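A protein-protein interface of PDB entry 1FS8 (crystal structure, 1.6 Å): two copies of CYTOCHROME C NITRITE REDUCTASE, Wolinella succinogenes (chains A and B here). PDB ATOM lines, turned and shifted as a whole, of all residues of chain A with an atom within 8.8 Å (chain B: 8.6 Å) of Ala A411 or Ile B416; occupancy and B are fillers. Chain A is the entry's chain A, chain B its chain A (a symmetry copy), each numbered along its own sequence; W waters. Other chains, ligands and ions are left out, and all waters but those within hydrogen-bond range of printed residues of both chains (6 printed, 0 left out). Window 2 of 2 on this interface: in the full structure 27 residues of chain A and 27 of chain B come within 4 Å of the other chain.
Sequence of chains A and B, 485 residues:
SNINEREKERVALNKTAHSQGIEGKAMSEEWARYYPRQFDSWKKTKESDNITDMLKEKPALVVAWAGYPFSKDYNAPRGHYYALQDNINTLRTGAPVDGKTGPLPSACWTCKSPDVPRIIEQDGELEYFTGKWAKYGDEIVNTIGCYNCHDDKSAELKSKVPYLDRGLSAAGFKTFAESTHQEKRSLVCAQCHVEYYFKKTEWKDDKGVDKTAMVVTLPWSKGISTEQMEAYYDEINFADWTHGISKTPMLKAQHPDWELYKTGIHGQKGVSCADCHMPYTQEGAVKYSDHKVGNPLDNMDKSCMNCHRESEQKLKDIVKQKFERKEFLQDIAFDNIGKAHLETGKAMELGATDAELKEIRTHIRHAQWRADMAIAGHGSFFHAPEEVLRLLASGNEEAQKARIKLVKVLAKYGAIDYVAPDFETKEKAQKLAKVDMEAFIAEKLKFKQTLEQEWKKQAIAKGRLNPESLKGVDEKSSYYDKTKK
Water W2 bridges NZ of Lys B408 and O of Tyr A418. Water W4 lies within hydrogen-bond range of the side-chain amino group of Lys A408 and the backbone carbonyl oxygen of Tyr B418. Water W5 lies within hydrogen-bond range of the side-chain carboxylate (OD1) of Asp B417 (2.7 Å) and the side-chain amino group (NZ) of Lys A408 (2.9 Å). Water W1 bridges the side-chain carboxylate (OD1) of Asp A417 and the side-chain amino group (NZ) of Lys B408. Water W6 lies within hydrogen-bond range of O of Tyr A418 (2.8 Å), O of Ile A416 (2.8 Å) and NZ of Lys B408 (3.1 Å). Water W3 lies within hydrogen-bond range of O of Tyr B418 (2.8 Å), O of Ile B416 (2.8 Å) and NZ of Lys A408 (3.1 Å).
Hydrophobic or aromatic side chains of chain B within 4 Å of the printed part of chain A: Val B407, Ala B411 and Ile B416. Hydrophobic or aromatic side chains of chain A within 4 Å of the printed part of chain B: Val A407, Ala A411 and Ile A416. Among the printed residues, 5 pairs touch across the chains.
Val B407 touches Val A407 (CG1 to CG1, 3.1 Å). Ala A411 touches Ile B416 (CB to CD1, 3.4 Å). CB of Ala B411 touches CD1 of Ile A416, 3.4 Å away.
Val B407 touches its own counterpart, Val A407. Lys A408 touches Ile B416, and with the chains exchanged Ile A416 touches Lys B408. Ala A411 touches Ile B416, and with the chains exchanged Ile A416 touches Ala B411. 17 positions are printed for both chains. Of the 5 pairs that touch across the chains among the printed residues, 5 have their exchanged pair printed and touching as well.
Ala A411 touches just one residue of chain B: Ile B416. Of chain A, only Lys A408 (3.3 Å) and Ala A411 (3.4 Å) come within 4 Å of Ile B416. Printed residues of chain A within 4 Å of Lys B408: Ile A416 (3.3 Å). Of the printed residues of chain A, Val B407 touches Val A407 (3.1 Å). Of the printed residues of chain B, Lys A408 touches Ile B416 (3.3 Å). Lys A405 touches none of the printed residues of chain B. The nearest printed residue of chain A that does not touch Ala B411 is Ala A411 (5.4 Å).
The backbone carbonyl oxygen (O) of Ile A416 sits close to the side-chain amino group (NZ) of Lys B408, 3.5 Å away. NZ of Lys A408 lies close to O of Ile B416 (3.5 Å).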
ATOM      1  N   GLU A 343       2.225  -8.431 -38.018  1.00  0.00           N
ATOM      2  CA  GLU A 343       3.198  -7.753 -37.173  1.00  0.00           C
ATOM      3  C   GLU A 343       4.127  -6.897 -38.022  1.00  0.00           C
ATOM      4  O   GLU A 343       4.590  -5.851 -37.581  1.00  0.00           O
ATOM      5  CB  GLU A 343       3.977  -8.787 -36.352  1.00  0.00           C
ATOM      6  CG  GLU A 343       3.055  -9.537 -35.400  1.00  0.00           C
ATOM      7  CD  GLU A 343       3.652 -10.805 -34.830  1.00  0.00           C
ATOM      8  OE1 GLU A 343       4.620 -11.336 -35.412  1.00  0.00           O
ATOM      9  OE2 GLU A 343       3.126 -11.284 -33.803  1.00  0.00           O
ATOM     10  N   LYS A 346       2.204  -3.841 -38.892  1.00  0.00           N
ATOM     11  CA  LYS A 346       2.140  -2.955 -37.731  1.00  0.00           C
ATOM     12  C   LYS A 346       3.452  -2.182 -37.633  1.00  0.00           C
ATOM     13  O   LYS A 346       3.451  -0.970 -37.418  1.00  0.00           O
ATOM     14  CB  LYS A 346       1.925  -3.764 -36.451  1.00  0.00           C
ATOM     15  CG  LYS A 346       1.966  -2.936 -35.158  1.00  0.00           C
ATOM     16  CD  LYS A 346       0.846  -1.908 -35.103  1.00  0.00           C
ATOM     17  CE  LYS A 346       0.828  -1.195 -33.756  1.00  0.00           C
ATOM     18  NZ  LYS A 346      -0.299  -0.222 -33.664  1.00  0.00           N
ATOM     19  N   ALA A 347       4.569  -2.888 -37.789  1.00  0.00           N
ATOM     20  CA  ALA A 347       5.881  -2.246 -37.733  1.00  0.00           C
ATOM     21  C   ALA A 347       5.963  -1.159 -38.800  1.00  0.00           C
ATOM     22  O   ALA A 347       6.514  -0.082 -38.562  1.00  0.00           O
ATOM     23  CB  ALA A 347       6.985  -3.278 -37.953  1.00  0.00           C
ATOM     24  N   LEU A 350       4.235   1.978 -37.848  1.00  0.00           N
ATOM     25  CA  LEU A 350       4.992   2.702 -36.836  1.00  0.00           C
ATOM     26  C   LEU A 350       6.225   3.414 -37.379  1.00  0.00           C
ATOM     27  O   LEU A 350       6.822   4.237 -36.683  1.00  0.00           O
ATOM     28  CB  LEU A 350       5.394   1.747 -35.711  1.00  0.00           C
ATOM     29  CG  LEU A 350       4.226   1.156 -34.914  1.00  0.00           C
ATOM     30  CD1 LEU A 350       4.731   0.051 -34.006  1.00  0.00           C
ATOM     31  CD2 LEU A 350       3.545   2.257 -34.103  1.00  0.00           C
ATOM     32  N   ILE A 404      10.387 -13.676 -34.152  1.00  0.00           N
ATOM     33  CA  ILE A 404      11.316 -13.345 -33.076  1.00  0.00           C
ATOM     34  C   ILE A 404      11.977 -12.009 -33.412  1.00  0.00           C
ATOM     35  O   ILE A 404      12.163 -11.160 -32.541  1.00  0.00           O
ATOM     36  CB  ILE A 404      12.392 -14.444 -32.906  1.00  0.00           C
ATOM     37  CG1 ILE A 404      11.761 -15.671 -32.242  1.00  0.00           C
ATOM     38  CG2 ILE A 404      13.565 -13.926 -32.062  1.00  0.00           C
ATOM     39  CD1 ILE A 404      12.685 -16.863 -32.154  1.00  0.00           C
ATOM     40  N   LYS A 405      12.324 -11.822 -34.681  1.00  0.00           N
ATOM     41  CA  LYS A 405      12.946 -10.574 -35.110  1.00  0.00           C
ATOM     42  C   LYS A 405      11.939  -9.425 -35.079  1.00  0.00           C
ATOM     43  O   LYS A 405      12.297  -8.284 -34.773  1.00  0.00           O
ATOM     44  CB  LYS A 405      13.540 -10.736 -36.514  1.00  0.00           C
ATOM     45  CG  LYS A 405      14.776 -11.632 -36.530  1.00  0.00           C
ATOM     46  CD  LYS A 405      15.341 -11.837 -37.926  1.00  0.00           C
ATOM     47  CE  LYS A 405      16.563 -12.752 -37.886  1.00  0.00           C
ATOM     48  NZ  LYS A 405      17.147 -12.993 -39.236  1.00  0.00           N
ATOM     49  N   LEU A 406      10.677  -9.725 -35.379  1.00  0.00           N
ATOM     50  CA  LEU A 406       9.634  -8.697 -35.364  1.00  0.00           C
ATOM     51  C   LEU A 406       9.388  -8.157 -33.958  1.00  0.00           C
ATOM     52  O   LEU A 406       9.014  -6.999 -33.794  1.00  0.00           O
ATOM     53  CB  LEU A 406       8.327  -9.246 -35.943  1.00  0.00           C
ATOM     54  CG  LEU A 406       8.245  -9.270 -37.471  1.00  0.00           C
ATOM     55  CD1 LEU A 406       7.147 -10.226 -37.913  1.00  0.00           C
ATOM     56  CD2 LEU A 406       7.991  -7.859 -38.001  1.00  0.00           C
ATOM     57  N   VAL A 407       9.591  -8.989 -32.941  1.00  0.00           N
ATOM     58  CA  VAL A 407       9.387  -8.531 -31.571  1.00  0.00           C
ATOM     59  C   VAL A 407      10.345  -7.376 -31.297  1.00  0.00           C
ATOM     60  O   VAL A 407       9.983  -6.380 -30.665  1.00  0.00           O
ATOM     61  CB  VAL A 407       9.667  -9.646 -30.536  1.00  0.00           C
ATOM     62  CG1 VAL A 407       9.542  -9.079 -29.116  1.00  0.00           C
ATOM     63  CG2 VAL A 407       8.690 -10.796 -30.729  1.00  0.00           C
ATOM     64  N   LYS A 408      11.570  -7.510 -31.789  1.00  0.00           N
ATOM     65  CA  LYS A 408      12.581  -6.484 -31.582  1.00  0.00           C
ATOM     66  C   LYS A 408      12.305  -5.213 -32.372  1.00  0.00           C
ATOM     67  O   LYS A 408      12.544  -4.113 -31.874  1.00  0.00           O
ATOM     68  CB  LYS A 408      13.957  -7.046 -31.927  1.00  0.00           C
ATOM     69  CG  LYS A 408      14.275  -8.287 -31.117  1.00  0.00           C
ATOM     70  CD  LYS A 408      15.666  -8.805 -31.384  1.00  0.00           C
ATOM     71  CE  LYS A 408      15.938 -10.048 -30.555  1.00  0.00           C
ATOM     72  NZ  LYS A 408      17.348 -10.490 -30.708  1.00  0.00           N
ATOM     73  N   VAL A 409      11.808  -5.353 -33.598  1.00  0.00           N
ATOM     74  CA  VAL A 409      11.492  -4.180 -34.406  1.00  0.00           C
ATOM     75  C   VAL A 409      10.317  -3.451 -33.763  1.00  0.00           C
ATOM     76  O   VAL A 409      10.327  -2.226 -33.633  1.00  0.00           O
ATOM     77  CB  VAL A 409      11.118  -4.563 -35.851  1.00  0.00           C
ATOM     78  CG1 VAL A 409      10.685  -3.324 -36.622  1.00  0.00           C
ATOM     79  CG2 VAL A 409      12.315  -5.206 -36.542  1.00  0.00           C
ATOM     80  N   LEU A 410       9.301  -4.208 -33.363  1.00  0.00           N
ATOM     81  CA  LEU A 410       8.135  -3.614 -32.721  1.00  0.00           C
ATOM     82  C   LEU A 410       8.560  -2.908 -31.436  1.00  0.00           C
ATOM     83  O   LEU A 410       8.103  -1.800 -31.145  1.00  0.00           O
ATOM     84  CB  LEU A 410       7.093  -4.693 -32.412  1.00  0.00           C
ATOM     85  CG  LEU A 410       6.371  -5.251 -33.644  1.00  0.00           C
ATOM     86  CD1 LEU A 410       5.529  -6.463 -33.255  1.00  0.00           C
ATOM     87  CD2 LEU A 410       5.494  -4.164 -34.254  1.00  0.00           C
ATOM     88  N   ALA A 411       9.446  -3.541 -30.675  1.00  0.00           N
ATOM     89  CA  ALA A 411       9.922  -2.952 -29.425  1.00  0.00           C
ATOM     90  C   ALA A 411      10.618  -1.622 -29.683  1.00  0.00           C
ATOM     91  O   ALA A 411      10.445  -0.667 -28.925  1.00  0.00           O
ATOM     92  CB  ALA A 411      10.874  -3.907 -28.716  1.00  0.00           C
ATOM     93  N   LYS A 412      11.404  -1.564 -30.753  1.00  0.00           N
ATOM     94  CA  LYS A 412      12.121  -0.340 -31.094  1.00  0.00           C
ATOM     95  C   LYS A 412      11.158   0.818 -31.309  1.00  0.00           C
ATOM     96  O   LYS A 412      11.461   1.963 -30.966  1.00  0.00           O
ATOM     97  CB  LYS A 412      12.966  -0.539 -32.357  1.00  0.00           C
ATOM     98  CG  LYS A 412      13.559   0.764 -32.881  1.00  0.00           C
ATOM     99  CD  LYS A 412      14.458   0.563 -34.087  1.00  0.00           C
ATOM    100  CE  LYS A 412      14.871   1.910 -34.656  1.00  0.00           C
ATOM    101  NZ  LYS A 412      15.885   1.787 -35.729  1.00  0.00           N
ATOM    102  N   TYR A 413       9.991   0.519 -31.867  1.00  0.00           N
ATOM    103  CA  TYR A 413       9.002   1.550 -32.128  1.00  0.00           C
ATOM    104  C   TYR A 413       7.936   1.661 -31.044  1.00  0.00           C
ATOM    105  O   TYR A 413       6.884   2.271 -31.249  1.00  0.00           O
ATOM    106  CB  TYR A 413       8.385   1.325 -33.508  1.00  0.00           C
ATOM    107  CG  TYR A 413       9.375   1.628 -34.613  1.00  0.00           C
ATOM    108  CD1 TYR A 413       9.639   2.942 -34.993  1.00  0.00           C
ATOM    109  CD2 TYR A 413      10.105   0.610 -35.220  1.00  0.00           C
ATOM    110  CE1 TYR A 413      10.612   3.237 -35.948  1.00  0.00           C
ATOM    111  CE2 TYR A 413      11.083   0.891 -36.176  1.00  0.00           C
ATOM    112  CZ  TYR A 413      11.330   2.208 -36.532  1.00  0.00           C
ATOM    113  OH  TYR A 413      12.304   2.501 -37.459  1.00  0.00           O
ATOM    114  N   GLY A 414       8.229   1.069 -29.889  1.00  0.00           N
ATOM    115  CA  GLY A 414       7.334   1.140 -28.745  1.00  0.00           C
ATOM    116  C   GLY A 414       6.094   0.267 -28.713  1.00  0.00           C
ATOM    117  O   GLY A 414       5.180   0.536 -27.934  1.00  0.00           O
ATOM    118  N   ALA A 415       6.054  -0.781 -29.531  1.00  0.00           N
ATOM    119  CA  ALA A 415       4.888  -1.660 -29.564  1.00  0.00           C
ATOM    120  C   ALA A 415       5.226  -3.123 -29.280  1.00  0.00           C
ATOM    121  O   ALA A 415       4.684  -4.019 -29.922  1.00  0.00           O
ATOM    122  CB  ALA A 415       4.200  -1.547 -30.917  1.00  0.00           C
ATOM    123  N   ILE A 416       6.096  -3.367 -28.305  1.00  0.00           N
ATOM    124  CA  ILE A 416       6.495  -4.735 -27.983  1.00  0.00           C
ATOM    125  C   ILE A 416       5.329  -5.622 -27.547  1.00  0.00           C
ATOM    126  O   ILE A 416       5.362  -6.836 -27.749  1.00  0.00           O
ATOM    127  CB  ILE A 416       7.580  -4.760 -26.877  1.00  0.00           C
ATOM    128  CG1 ILE A 416       8.314  -6.107 -26.901  1.00  0.00           C
ATOM    129  CG2 ILE A 416       6.945  -4.547 -25.502  1.00  0.00           C
ATOM    130  CD1 ILE A 416       9.531  -6.157 -25.999  1.00  0.00           C
ATOM    131  N   ASP A 417       4.302  -5.019 -26.954  1.00  0.00           N
ATOM    132  CA  ASP A 417       3.142  -5.777 -26.490  1.00  0.00           C
ATOM    133  C   ASP A 417       2.015  -5.856 -27.513  1.00  0.00           C
ATOM    134  O   ASP A 417       0.887  -6.211 -27.172  1.00  0.00           O
ATOM    135  CB  ASP A 417       2.601  -5.179 -25.193  1.00  0.00           C
ATOM    136  CG  ASP A 417       3.605  -5.246 -24.062  1.00  0.00           C
ATOM    137  OD1 ASP A 417       4.142  -6.347 -23.815  1.00  0.00           O
ATOM    138  OD2 ASP A 417       3.853  -4.201 -23.422  1.00  0.00           O
ATOM    139  N   TYR A 418       2.317  -5.516 -28.762  1.00  0.00           N
ATOM    140  CA  TYR A 418       1.325  -5.570 -29.829  1.00  0.00           C
ATOM    141  C   TYR A 418       0.842  -7.000 -30.033  1.00  0.00           C
ATOM    142  O   TYR A 418       1.642  -7.938 -30.057  1.00  0.00           O
ATOM    143  CB  TYR A 418       1.930  -5.062 -31.139  1.00  0.00           C
ATOM    144  CG  TYR A 418       1.059  -5.283 -32.360  1.00  0.00           C
ATOM    145  CD1 TYR A 418      -0.118  -4.555 -32.549  1.00  0.00           C
ATOM    146  CD2 TYR A 418       1.420  -6.211 -33.336  1.00  0.00           C
ATOM    147  CE1 TYR A 418      -0.910  -4.747 -33.685  1.00  0.00           C
ATOM    148  CE2 TYR A 418       0.638  -6.409 -34.470  1.00  0.00           C
ATOM    149  CZ  TYR A 418      -0.524  -5.674 -34.641  1.00  0.00           C
ATOM    150  OH  TYR A 418      -1.284  -5.867 -35.774  1.00  0.00           O
ATOM    151  N   GLU B 343      18.307 -18.340 -22.711  1.00  0.00           N
ATOM    152  CA  GLU B 343      17.659 -17.039 -22.616  1.00  0.00           C
ATOM    153  C   GLU B 343      16.888 -16.930 -21.308  1.00  0.00           C
ATOM    154  O   GLU B 343      16.774 -15.849 -20.739  1.00  0.00           O
ATOM    155  CB  GLU B 343      16.745 -16.830 -23.829  1.00  0.00           C
ATOM    156  CG  GLU B 343      17.548 -16.797 -25.121  1.00  0.00           C
ATOM    157  CD  GLU B 343      16.716 -16.965 -26.373  1.00  0.00           C
ATOM    158  OE1 GLU B 343      15.578 -17.469 -26.283  1.00  0.00           O
ATOM    159  OE2 GLU B 343      17.222 -16.610 -27.459  1.00  0.00           O
ATOM    160  N   LYS B 346      19.421 -16.269 -18.672  1.00  0.00           N
ATOM    161  CA  LYS B 346      19.858 -14.876 -18.751  1.00  0.00           C
ATOM    162  C   LYS B 346      18.817 -13.998 -18.065  1.00  0.00           C
ATOM    163  O   LYS B 346      19.162 -13.112 -17.283  1.00  0.00           O
ATOM    164  CB  LYS B 346      20.011 -14.444 -20.211  1.00  0.00           C
ATOM    165  CG  LYS B 346      20.350 -12.960 -20.405  1.00  0.00           C
ATOM    166  CD  LYS B 346      21.697 -12.598 -19.799  1.00  0.00           C
ATOM    167  CE  LYS B 346      22.069 -11.155 -20.123  1.00  0.00           C
ATOM    168  NZ  LYS B 346      23.414 -10.799 -19.583  1.00  0.00           N
ATOM    169  N   LEU B 350      19.131 -11.473 -14.674  1.00  0.00           N
ATOM    170  CA  LEU B 350      18.721 -10.075 -14.678  1.00  0.00           C
ATOM    171  C   LEU B 350      17.661  -9.739 -13.638  1.00  0.00           C
ATOM    172  O   LEU B 350      17.391  -8.564 -13.384  1.00  0.00           O
ATOM    173  CB  LEU B 350      18.227  -9.687 -16.073  1.00  0.00           C
ATOM    174  CG  LEU B 350      19.289  -9.741 -17.176  1.00  0.00           C
ATOM    175  CD1 LEU B 350      18.629  -9.579 -18.532  1.00  0.00           C
ATOM    176  CD2 LEU B 350      20.330  -8.647 -16.945  1.00  0.00           C
ATOM    177  N   ILE B 404       9.603 -16.400 -28.146  1.00  0.00           N
ATOM    178  CA  ILE B 404       8.935 -15.143 -28.468  1.00  0.00           C
ATOM    179  C   ILE B 404       8.610 -14.428 -27.158  1.00  0.00           C
ATOM    180  O   ILE B 404       8.763 -13.212 -27.048  1.00  0.00           O
ATOM    181  CB  ILE B 404       7.638 -15.388 -29.276  1.00  0.00           C
ATOM    182  CG1 ILE B 404       8.003 -15.783 -30.710  1.00  0.00           C
ATOM    183  CG2 ILE B 404       6.756 -14.131 -29.278  1.00  0.00           C
ATOM    184  CD1 ILE B 404       6.817 -16.184 -31.557  1.00  0.00           C
ATOM    185  N   LEU B 406      10.207 -14.897 -24.329  1.00  0.00           N
ATOM    186  CA  LEU B 406      11.476 -14.545 -23.689  1.00  0.00           C
ATOM    187  C   LEU B 406      12.028 -13.221 -24.209  1.00  0.00           C
ATOM    188  O   LEU B 406      12.711 -12.503 -23.482  1.00  0.00           O
ATOM    189  CB  LEU B 406      12.511 -15.655 -23.897  1.00  0.00           C
ATOM    190  CG  LEU B 406      12.393 -16.849 -22.948  1.00  0.00           C
ATOM    191  CD1 LEU B 406      13.139 -18.042 -23.527  1.00  0.00           C
ATOM    192  CD2 LEU B 406      12.941 -16.476 -21.570  1.00  0.00           C
ATOM    193  N   VAL B 407      11.743 -12.893 -25.465  1.00  0.00           N
ATOM    194  CA  VAL B 407      12.228 -11.634 -26.020  1.00  0.00           C
ATOM    195  C   VAL B 407      11.649 -10.486 -25.199  1.00  0.00           C
ATOM    196  O   VAL B 407      12.335  -9.507 -24.894  1.00  0.00           O
ATOM    197  CB  VAL B 407      11.797 -11.441 -27.492  1.00  0.00           C
ATOM    198  CG1 VAL B 407      12.242 -10.058 -27.987  1.00  0.00           C
ATOM    199  CG2 VAL B 407      12.408 -12.529 -28.363  1.00  0.00           C
ATOM    200  N   LYS B 408      10.380 -10.618 -24.834  1.00  0.00           N
ATOM    201  CA  LYS B 408       9.707  -9.584 -24.062  1.00  0.00           C
ATOM    202  C   LYS B 408      10.205  -9.497 -22.627  1.00  0.00           C
ATOM    203  O   LYS B 408      10.327  -8.400 -22.082  1.00  0.00           O
ATOM    204  CB  LYS B 408       8.200  -9.821 -24.097  1.00  0.00           C
ATOM    205  CG  LYS B 408       7.671  -9.864 -25.517  1.00  0.00           C
ATOM    206  CD  LYS B 408       6.171 -10.011 -25.566  1.00  0.00           C
ATOM    207  CE  LYS B 408       5.688 -10.053 -27.005  1.00  0.00           C
ATOM    208  NZ  LYS B 408       4.204 -10.063 -27.067  1.00  0.00           N
ATOM    209  N   VAL B 409      10.492 -10.641 -22.011  1.00  0.00           N
ATOM    210  CA  VAL B 409      11.001 -10.636 -20.644  1.00  0.00           C
ATOM    211  C   VAL B 409      12.396 -10.022 -20.649  1.00  0.00           C
ATOM    212  O   VAL B 409      12.724  -9.189 -19.802  1.00  0.00           O
ATOM    213  CB  VAL B 409      11.079 -12.059 -20.056  1.00  0.00           C
ATOM    214  CG1 VAL B 409      11.722 -12.018 -18.677  1.00  0.00           C
ATOM    215  CG2 VAL B 409       9.679 -12.654 -19.954  1.00  0.00           C
ATOM    216  N   LEU B 410      13.220 -10.437 -21.605  1.00  0.00           N
ATOM    217  CA  LEU B 410      14.571  -9.900 -21.711  1.00  0.00           C
ATOM    218  C   LEU B 410      14.510  -8.392 -21.944  1.00  0.00           C
ATOM    219  O   LEU B 410      15.273  -7.630 -21.347  1.00  0.00           O
ATOM    220  CB  LEU B 410      15.324 -10.582 -22.856  1.00  0.00           C
ATOM    221  CG  LEU B 410      15.716 -12.039 -22.581  1.00  0.00           C
ATOM    222  CD1 LEU B 410      16.253 -12.687 -23.854  1.00  0.00           C
ATOM    223  CD2 LEU B 410      16.765 -12.082 -21.476  1.00  0.00           C
ATOM    224  N   ALA B 411      13.591  -7.961 -22.801  1.00  0.00           N
ATOM    225  CA  ALA B 411      13.445  -6.537 -23.095  1.00  0.00           C
ATOM    226  C   ALA B 411      13.095  -5.757 -21.834  1.00  0.00           C
ATOM    227  O   ALA B 411      13.605  -4.657 -21.616  1.00  0.00           O
ATOM    228  CB  ALA B 411      12.372  -6.320 -24.154  1.00  0.00           C
ATOM    229  N   LYS B 412      12.225  -6.328 -21.008  1.00  0.00           N
ATOM    230  CA  LYS B 412      11.817  -5.668 -19.772  1.00  0.00           C
ATOM    231  C   LYS B 412      13.015  -5.392 -18.876  1.00  0.00           C
ATOM    232  O   LYS B 412      13.067  -4.369 -18.189  1.00  0.00           O
ATOM    233  CB  LYS B 412      10.799  -6.523 -19.010  1.00  0.00           C
ATOM    234  CG  LYS B 412      10.507  -5.988 -17.613  1.00  0.00           C
ATOM    235  CD  LYS B 412       9.444  -6.787 -16.882  1.00  0.00           C
ATOM    236  CE  LYS B 412       9.332  -6.307 -15.444  1.00  0.00           C
ATOM    237  NZ  LYS B 412       8.195  -6.928 -14.726  1.00  0.00           N
ATOM    238  N   TYR B 413      13.984  -6.300 -18.891  1.00  0.00           N
ATOM    239  CA  TYR B 413      15.168  -6.141 -18.065  1.00  0.00           C
ATOM    240  C   TYR B 413      16.352  -5.532 -18.807  1.00  0.00           C
ATOM    241  O   TYR B 413      17.493  -5.599 -18.344  1.00  0.00           O
ATOM    242  CB  TYR B 413      15.528  -7.485 -17.430  1.00  0.00           C
ATOM    243  CG  TYR B 413      14.522  -7.882 -16.370  1.00  0.00           C
ATOM    244  CD1 TYR B 413      14.567  -7.317 -15.097  1.00  0.00           C
ATOM    245  CD2 TYR B 413      13.482  -8.759 -16.663  1.00  0.00           C
ATOM    246  CE1 TYR B 413      13.594  -7.610 -14.142  1.00  0.00           C
ATOM    247  CE2 TYR B 413      12.500  -9.060 -15.716  1.00  0.00           C
ATOM    248  CZ  TYR B 413      12.565  -8.479 -14.458  1.00  0.00           C
ATOM    249  OH  TYR B 413      11.594  -8.752 -13.523  1.00  0.00           O
ATOM    250  N   GLY B 414      16.061  -4.933 -19.958  1.00  0.00           N
ATOM    251  CA  GLY B 414      17.078  -4.257 -20.748  1.00  0.00           C
ATOM    252  C   GLY B 414      18.040  -5.078 -21.584  1.00  0.00           C
ATOM    253  O   GLY B 414      19.082  -4.566 -21.993  1.00  0.00           O
ATOM    254  N   ALA B 415      17.702  -6.335 -21.862  1.00  0.00           N
ATOM    255  CA  ALA B 415      18.583  -7.190 -22.652  1.00  0.00           C
ATOM    256  C   ALA B 415      17.913  -7.759 -23.901  1.00  0.00           C
ATOM    257  O   ALA B 415      18.116  -8.923 -24.238  1.00  0.00           O
ATOM    258  CB  ALA B 415      19.103  -8.329 -21.786  1.00  0.00           C
ATOM    259  N   ILE B 416      17.137  -6.937 -24.601  1.00  0.00           N
ATOM    260  CA  ILE B 416      16.437  -7.405 -25.796  1.00  0.00           C
ATOM    261  C   ILE B 416      17.375  -7.908 -26.892  1.00  0.00           C
ATOM    262  O   ILE B 416      17.000  -8.778 -27.680  1.00  0.00           O
ATOM    263  CB  ILE B 416      15.530  -6.297 -26.387  1.00  0.00           C
ATOM    264  CG1 ILE B 416      14.471  -6.926 -27.302  1.00  0.00           C
ATOM    265  CG2 ILE B 416      16.364  -5.293 -27.184  1.00  0.00           C
ATOM    266  CD1 ILE B 416      13.406  -5.954 -27.766  1.00  0.00           C
ATOM    267  N   ASP B 417      18.589  -7.368 -26.942  1.00  0.00           N
ATOM    268  CA  ASP B 417      19.558  -7.772 -27.958  1.00  0.00           C
ATOM    269  C   ASP B 417      20.490  -8.891 -27.504  1.00  0.00           C
ATOM    270  O   ASP B 417      21.518  -9.139 -28.132  1.00  0.00           O
ATOM    271  CB  ASP B 417      20.394  -6.573 -28.401  1.00  0.00           C
ATOM    272  CG  ASP B 417      19.557  -5.493 -29.051  1.00  0.00           C
ATOM    273  OD1 ASP B 417      18.786  -5.822 -29.977  1.00  0.00           O
ATOM    274  OD2 ASP B 417      19.673  -4.318 -28.637  1.00  0.00           O
ATOM    275  N   TYR B 418      20.134  -9.556 -26.409  1.00  0.00           N
ATOM    276  CA  TYR B 418      20.937 -10.658 -25.891  1.00  0.00           C
ATOM    277  C   TYR B 418      20.999 -11.791 -26.905  1.00  0.00           C
ATOM    278  O   TYR B 418      19.985 -12.161 -27.502  1.00  0.00           O
ATOM    279  CB  TYR B 418      20.328 -11.189 -24.593  1.00  0.00           C
ATOM    280  CG  TYR B 418      20.951 -12.475 -24.087  1.00  0.00           C
ATOM    281  CD1 TYR B 418      22.245 -12.493 -23.561  1.00  0.00           C
ATOM    282  CD2 TYR B 418      20.241 -13.675 -24.122  1.00  0.00           C
ATOM    283  CE1 TYR B 418      22.811 -13.676 -23.078  1.00  0.00           C
ATOM    284  CE2 TYR B 418      20.797 -14.858 -23.644  1.00  0.00           C
ATOM    285  CZ  TYR B 418      22.080 -14.854 -23.122  1.00  0.00           C
ATOM    286  OH  TYR B 418      22.616 -16.028 -22.638  1.00  0.00           O
ATOM    287  N   VAL B 419      22.192 -12.346 -27.088  1.00  0.00           N
ATOM    288  CA  VAL B 419      22.390 -13.451 -28.010  1.00  0.00           C
ATOM    289  C   VAL B 419      22.858 -14.659 -27.210  1.00  0.00           C
ATOM    290  O   VAL B 419      23.969 -14.669 -26.680  1.00  0.00           O
ATOM    291  CB  VAL B 419      23.448 -13.107 -29.080  1.00  0.00           C
ATOM    292  CG1 VAL B 419      23.636 -14.278 -30.034  1.00  0.00           C
ATOM    293  CG2 VAL B 419      23.017 -11.868 -29.842  1.00  0.00           C
ATOM    294  N   ALA B 420      22.000 -15.670 -27.110  1.00  0.00           N
ATOM    295  CA  ALA B 420      22.342 -16.872 -26.367  1.00  0.00           C
ATOM    296  C   ALA B 420      23.667 -17.429 -26.876  1.00  0.00           C
ATOM    297  O   ALA B 420      23.912 -17.473 -28.083  1.00  0.00           O
ATOM    298  CB  ALA B 420      21.237 -17.915 -26.522  1.00  0.00           C
HETATM  299  O   HOH W   1       3.235  -8.781 -24.679  1.00  0.00           O
HETATM  300  O   HOH W   2       1.899  -9.539 -28.016  1.00  0.00           O
HETATM  301  O   HOH W   3      17.264 -11.576 -27.846  1.00  0.00           O
HETATM  302  O   HOH W   4      19.573 -11.500 -29.990  1.00  0.00           O
HETATM  303  O   HOH W   5      18.908  -8.167 -31.384  1.00  0.00           O
HETATM  304  O   HOH W   6       4.356  -8.563 -29.732  1.00  0.00           O
